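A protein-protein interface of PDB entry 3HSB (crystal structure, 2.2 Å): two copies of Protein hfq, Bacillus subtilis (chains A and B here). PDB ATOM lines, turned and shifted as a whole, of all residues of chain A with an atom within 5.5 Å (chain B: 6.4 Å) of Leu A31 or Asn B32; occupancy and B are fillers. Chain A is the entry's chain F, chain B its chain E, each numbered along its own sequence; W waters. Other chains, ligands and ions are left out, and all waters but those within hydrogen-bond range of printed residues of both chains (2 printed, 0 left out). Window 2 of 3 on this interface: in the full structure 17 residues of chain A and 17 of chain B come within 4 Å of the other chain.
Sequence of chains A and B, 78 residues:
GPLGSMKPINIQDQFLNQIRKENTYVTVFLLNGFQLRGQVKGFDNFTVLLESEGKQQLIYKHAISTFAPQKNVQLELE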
ATOM      1  N   PHE A  29      -7.455  19.603  -5.454  1.00  0.00           N
ATOM      2  CA  PHE A  29      -7.439  18.572  -6.440  1.00  0.00           C
ATOM      3  C   PHE A  29      -6.222  18.839  -7.293  1.00  0.00           C
ATOM      4  O   PHE A  29      -6.084  19.928  -7.852  1.00  0.00           O
ATOM      5  CB  PHE A  29      -8.730  18.583  -7.301  1.00  0.00           C
ATOM      6  CG  PHE A  29      -9.981  18.243  -6.505  1.00  0.00           C
ATOM      7  CD1 PHE A  29     -10.467  16.908  -6.474  1.00  0.00           C
ATOM      8  CD2 PHE A  29     -10.649  19.216  -5.720  1.00  0.00           C
ATOM      9  CE1 PHE A  29     -11.623  16.556  -5.723  1.00  0.00           C
ATOM     10  CE2 PHE A  29     -11.821  18.891  -5.008  1.00  0.00           C
ATOM     11  CZ  PHE A  29     -12.302  17.573  -4.990  1.00  0.00           C
ATOM     12  N   LEU A  30      -5.376  17.859  -7.428  1.00  0.00           N
ATOM     13  CA  LEU A  30      -4.117  18.099  -8.128  1.00  0.00           C
ATOM     14  C   LEU A  30      -4.337  17.879  -9.611  1.00  0.00           C
ATOM     15  O   LEU A  30      -5.343  17.275  -9.972  1.00  0.00           O
ATOM     16  CB  LEU A  30      -3.045  17.185  -7.557  1.00  0.00           C
ATOM     17  CG  LEU A  30      -2.716  17.529  -6.054  1.00  0.00           C
ATOM     18  CD1 LEU A  30      -1.499  16.737  -5.493  1.00  0.00           C
ATOM     19  CD2 LEU A  30      -2.498  19.006  -5.688  1.00  0.00           C
ATOM     20  N   LEU A  31      -3.400  18.278 -10.459  1.00  0.00           N
ATOM     21  CA  LEU A  31      -3.485  18.036 -11.899  1.00  0.00           C
ATOM     22  C   LEU A  31      -3.541  16.571 -12.323  1.00  0.00           C
ATOM     23  O   LEU A  31      -4.064  16.230 -13.403  1.00  0.00           O
ATOM     24  CB  LEU A  31      -2.236  18.599 -12.536  1.00  0.00           C
ATOM     25  CG  LEU A  31      -2.217  19.906 -13.320  1.00  0.00           C
ATOM     26  CD1 LEU A  31      -0.761  19.945 -14.023  1.00  0.00           C
ATOM     27  CD2 LEU A  31      -3.377  20.121 -14.303  1.00  0.00           C
ATOM     28  N   ASN A  32      -2.891  15.733 -11.537  1.00  0.00           N
ATOM     29  CA  ASN A  32      -2.915  14.287 -11.688  1.00  0.00           C
ATOM     30  C   ASN A  32      -4.155  13.617 -11.063  1.00  0.00           C
ATOM     31  O   ASN A  32      -4.221  12.397 -10.986  1.00  0.00           O
ATOM     32  CB  ASN A  32      -1.589  13.638 -11.185  1.00  0.00           C
ATOM     33  CG  ASN A  32      -1.490  13.520  -9.645  1.00  0.00           C
ATOM     34  OD1 ASN A  32      -2.334  14.031  -8.886  1.00  0.00           O
ATOM     35  ND2 ASN A  32      -0.412  12.863  -9.187  1.00  0.00           N
ATOM     36  N   GLY A  33      -5.117  14.414 -10.604  1.00  0.00           N
ATOM     37  CA  GLY A  33      -6.321  13.855  -9.999  1.00  0.00           C
ATOM     38  C   GLY A  33      -6.173  13.375  -8.561  1.00  0.00           C
ATOM     39  O   GLY A  33      -7.188  12.981  -7.982  1.00  0.00           O
ATOM     40  N   HIS A  62       1.206  25.435  -9.997  1.00  0.00           N
ATOM     41  CA  HIS A  62       1.146  24.792 -11.331  1.00  0.00           C
ATOM     42  C   HIS A  62       0.708  23.356 -11.269  1.00  0.00           C
ATOM     43  O   HIS A  62       0.269  22.769 -12.294  1.00  0.00           O
ATOM     44  CB  HIS A  62       2.472  24.920 -12.180  1.00  0.00           C
ATOM     45  CG  HIS A  62       3.659  24.233 -11.548  1.00  0.00           C
ATOM     46  ND1 HIS A  62       4.801  24.894 -11.228  1.00  0.00           N
ATOM     47  CD2 HIS A  62       3.878  22.944 -11.208  1.00  0.00           C
ATOM     48  CE1 HIS A  62       5.674  24.071 -10.686  1.00  0.00           C
ATOM     49  NE2 HIS A  62       5.135  22.869 -10.664  1.00  0.00           N
ATOM     50  N   ALA A  63       0.759  22.735 -10.095  1.00  0.00           N
ATOM     51  CA  ALA A  63       0.337  21.321 -10.023  1.00  0.00           C
ATOM     52  C   ALA A  63      -1.086  21.212  -9.464  1.00  0.00           C
ATOM     53  O   ALA A  63      -1.577  20.085  -9.264  1.00  0.00           O
ATOM     54  CB  ALA A  63       1.203  20.579  -9.149  1.00  0.00           C
ATOM     55  N   ILE A  64      -1.721  22.343  -9.159  1.00  0.00           N
ATOM     56  CA  ILE A  64      -3.048  22.317  -8.583  1.00  0.00           C
ATOM     57  C   ILE A  64      -4.039  22.568  -9.730  1.00  0.00           C
ATOM     58  O   ILE A  64      -3.829  23.391 -10.650  1.00  0.00           O
ATOM     59  CB  ILE A  64      -3.270  23.423  -7.495  1.00  0.00           C
ATOM     60  CG1 ILE A  64      -2.369  23.206  -6.308  1.00  0.00           C
ATOM     61  CG2 ILE A  64      -4.760  23.454  -7.128  1.00  0.00           C
ATOM     62  CD1 ILE A  64      -2.189  24.379  -5.185  1.00  0.00           C
ATOM     63  N   SER A  65      -5.144  21.901  -9.611  1.00  0.00           N
ATOM     64  CA  SER A  65      -6.268  22.064 -10.483  1.00  0.00           C
ATOM     65  C   SER A  65      -7.365  22.942  -9.789  1.00  0.00           C
ATOM     66  O   SER A  65      -7.730  24.016 -10.317  1.00  0.00           O
ATOM     67  CB  SER A  65      -6.699  20.646 -10.963  1.00  0.00           C
ATOM     68  OG  SER A  65      -7.988  20.799 -11.453  1.00  0.00           O
ATOM     69  N   LEU B  30     -11.574  19.848 -17.378  1.00  0.00           N
ATOM     70  CA  LEU B  30     -10.228  20.009 -16.820  1.00  0.00           C
ATOM     71  C   LEU B  30      -9.264  19.068 -17.462  1.00  0.00           C
ATOM     72  O   LEU B  30      -9.651  18.050 -18.013  1.00  0.00           O
ATOM     73  CB  LEU B  30     -10.250  19.854 -15.281  1.00  0.00           C
ATOM     74  CG  LEU B  30     -11.233  20.759 -14.555  1.00  0.00           C
ATOM     75  CD1 LEU B  30     -11.088  20.283 -13.152  1.00  0.00           C
ATOM     76  CD2 LEU B  30     -10.860  22.268 -14.612  1.00  0.00           C
ATOM     77  N   LEU B  31      -8.002  19.454 -17.498  1.00  0.00           N
ATOM     78  CA  LEU B  31      -6.979  18.637 -18.053  1.00  0.00           C
ATOM     79  C   LEU B  31      -6.838  17.258 -17.334  1.00  0.00           C
ATOM     80  O   LEU B  31      -6.524  16.275 -17.975  1.00  0.00           O
ATOM     81  CB  LEU B  31      -5.665  19.420 -18.096  1.00  0.00           C
ATOM     82  CG  LEU B  31      -5.499  20.345 -19.328  1.00  0.00           C
ATOM     83  CD1 LEU B  31      -4.410  21.348 -19.103  1.00  0.00           C
ATOM     84  CD2 LEU B  31      -5.156  19.527 -20.600  1.00  0.00           C
ATOM     85  N   ASN B  32      -7.083  17.201 -16.038  1.00  0.00           N
ATOM     86  CA  ASN B  32      -7.030  15.944 -15.231  1.00  0.00           C
ATOM     87  C   ASN B  32      -8.163  14.966 -15.526  1.00  0.00           C
ATOM     88  O   ASN B  32      -8.275  13.923 -14.835  1.00  0.00           O
ATOM     89  CB  ASN B  32      -6.956  16.260 -13.692  1.00  0.00           C
ATOM     90  CG  ASN B  32      -8.230  16.908 -13.149  1.00  0.00           C
ATOM     91  OD1 ASN B  32      -9.244  16.812 -13.806  1.00  0.00           O
ATOM     92  ND2 ASN B  32      -8.199  17.509 -11.894  1.00  0.00           N
ATOM     93  N   GLY B  33      -8.986  15.282 -16.526  1.00  0.00           N
ATOM     94  CA  GLY B  33     -10.009  14.373 -17.027  1.00  0.00           C
ATOM     95  C   GLY B  33     -11.375  14.680 -16.459  1.00  0.00           C
ATOM     96  O   GLY B  33     -12.409  14.205 -16.953  1.00  0.00           O
ATOM     97  N   PHE B  34     -11.380  15.465 -15.408  1.00  0.00           N
ATOM     98  CA  PHE B  34     -12.568  15.730 -14.716  1.00  0.00           C
ATOM     99  C   PHE B  34     -13.363  16.825 -15.423  1.00  0.00           C
ATOM    100  O   PHE B  34     -12.769  17.741 -16.029  1.00  0.00           O
ATOM    101  CB  PHE B  34     -12.204  16.118 -13.303  1.00  0.00           C
ATOM    102  CG  PHE B  34     -13.311  16.000 -12.359  1.00  0.00           C
ATOM    103  CD1 PHE B  34     -14.046  17.118 -12.004  1.00  0.00           C
ATOM    104  CD2 PHE B  34     -13.657  14.753 -11.831  1.00  0.00           C
ATOM    105  CE1 PHE B  34     -15.133  17.017 -11.115  1.00  0.00           C
ATOM    106  CE2 PHE B  34     -14.728  14.623 -10.942  1.00  0.00           C
ATOM    107  CZ  PHE B  34     -15.500  15.756 -10.598  1.00  0.00           C
ATOM    108  N   GLN B  35     -14.683  16.707 -15.410  1.00  0.00           N
ATOM    109  CA  GLN B  35     -15.493  17.799 -15.861  1.00  0.00           C
ATOM    110  C   GLN B  35     -16.548  18.192 -14.852  1.00  0.00           C
ATOM    111  O   GLN B  35     -17.211  17.318 -14.294  1.00  0.00           O
ATOM    112  CB  GLN B  35     -16.091  17.541 -17.231  1.00  0.00           C
ATOM    113  CG  GLN B  35     -17.219  16.557 -17.264  1.00  0.00           C
ATOM    114  CD  GLN B  35     -17.487  16.033 -18.672  1.00  0.00           C
ATOM    115  OE1 GLN B  35     -16.569  15.517 -19.312  1.00  0.00           O
ATOM    116  NE2 GLN B  35     -18.743  16.151 -19.157  1.00  0.00           N
ATOM    117  N   HIS B  62      -4.693  27.364 -15.807  1.00  0.00           N
ATOM    118  CA  HIS B  62      -3.746  26.349 -16.354  1.00  0.00           C
ATOM    119  C   HIS B  62      -4.299  24.960 -16.296  1.00  0.00           C
ATOM    120  O   HIS B  62      -3.797  24.103 -17.025  1.00  0.00           O
ATOM    121  CB  HIS B  62      -2.304  26.350 -15.685  1.00  0.00           C
ATOM    122  CG  HIS B  62      -2.291  26.060 -14.192  1.00  0.00           C
ATOM    123  ND1 HIS B  62      -2.003  27.013 -13.252  1.00  0.00           N
ATOM    124  CD2 HIS B  62      -2.550  24.925 -13.498  1.00  0.00           C
ATOM    125  CE1 HIS B  62      -2.048  26.479 -12.041  1.00  0.00           C
ATOM    126  NE2 HIS B  62      -2.446  25.228 -12.167  1.00  0.00           N
ATOM    127  N   ALA B  63      -5.337  24.677 -15.470  1.00  0.00           N
ATOM    128  CA  ALA B  63      -5.762  23.269 -15.277  1.00  0.00           C
ATOM    129  C   ALA B  63      -7.009  22.962 -16.183  1.00  0.00           C
ATOM    130  O   ALA B  63      -7.554  21.811 -16.214  1.00  0.00           O
ATOM    131  CB  ALA B  63      -6.137  23.091 -13.779  1.00  0.00           C
ATOM    132  N   ILE B  64      -7.471  24.002 -16.902  1.00  0.00           N
ATOM    133  CA  ILE B  64      -8.683  23.907 -17.691  1.00  0.00           C
ATOM    134  C   ILE B  64      -8.360  23.680 -19.166  1.00  0.00           C
ATOM    135  O   ILE B  64      -7.394  24.317 -19.725  1.00  0.00           O
ATOM    136  CB  ILE B  64      -9.547  25.216 -17.556  1.00  0.00           C
ATOM    137  CG1 ILE B  64     -10.037  25.428 -16.091  1.00  0.00           C
ATOM    138  CG2 ILE B  64     -10.770  25.152 -18.587  1.00  0.00           C
ATOM    139  CD1 ILE B  64     -10.793  26.847 -15.868  1.00  0.00           C
HETATM  140  O   HOH W   1      -6.703  19.797 -14.443  1.00  0.00           O
HETATM  141  O   HOH W   2      -6.436  12.262 -13.669  1.00  0.00           O
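The backbone NH of Leu B31 sits at hydrogen-bond distance from the backbone carbonyl oxygen of Ala B63 (2.7 Å). OD1 of Asn B32 sits at hydrogen-bond distance from N of Phe B34 (3.0 Å). O of Phe A29 is in hydrogen-bond range of N of Ser A65, 2.8 Å away. N of Leu A31 lies within hydrogen-bond range of O of Ala A63, 2.8 Å away.
Water W2 lies within hydrogen-bond range of O of Asn B32 (2.7 Å) and O of Asn A32 (3.5 Å). Water W1 lies within hydrogen-bond range of the backbone carbonyl oxygen (O) of Ala B63 (2.8 Å), the backbone NH (N) of Asn B32 (3.1 Å), the backbone NH (N) of Leu B31 (3.3 Å) and the side-chain hydroxyl (OG) of Ser A65 (3.4 Å).
Of the 9 printed residues of chain B, 4 touch a printed residue of chain A. Hydrophobic or aromatic side chains of chain B that line the printed part of chain A: Leu B30, His B62 and Ala B63.
Among the printed residues, pairs that only touch across the chains: Leu A31 with Asn B32 (2.9 Å), His A62 with His B62 (3.7 Å), Ile A64 with Ala B63 (3.9 Å), Ser A65 with Leu B30 (3.6 Å) and Ser A65 with Ala B63 (3.5 Å).
The side-chain amide nitrogen of Asn B32 sits at hydrogen-bond distance from the backbone carbonyl oxygen of Leu A30 (3.5 Å). ND2 of Asn B32 lies within hydrogen-bond range of OG of Ser A65 (3.3 Å). O of Ile A64 sits at hydrogen-bond distance from NE2 of His B62, 2.8 Å away.
Leu A31 touches just one residue of chain B: Asn B32. Asn B32 touches just these residues of chain A: Leu A30, Leu A31 and Ser A65. Of the printed residues of chain B, His A62 touches His B62. Printed residues of chain A within 4 Å of Ala B63: Ile A64 and Ser A65. Of the printed residues of chain A, Leu B30 touches Ser A65. Asn A32 touches none of the printed residues of chain B. The nearest residue of chain A that does not touch Asn B32 is Gly A33 (4.04 Å).
Leu A30 touches Asn B32, but with the chains exchanged Asn A32 does not touch Leu B30 (9.2 Å). Leu A31 touches Asn B32, but with the chains exchanged Asn A32 does not touch Leu B31 (7.2 Å). Ile A64 touches His B62, but with the chains exchanged His A62 does not touch Ile B64 (9.1 Å). Ile A64 touches Ala B63, but with the chains exchanged Ala A63 does not touch Ile B64 (10.2 Å).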
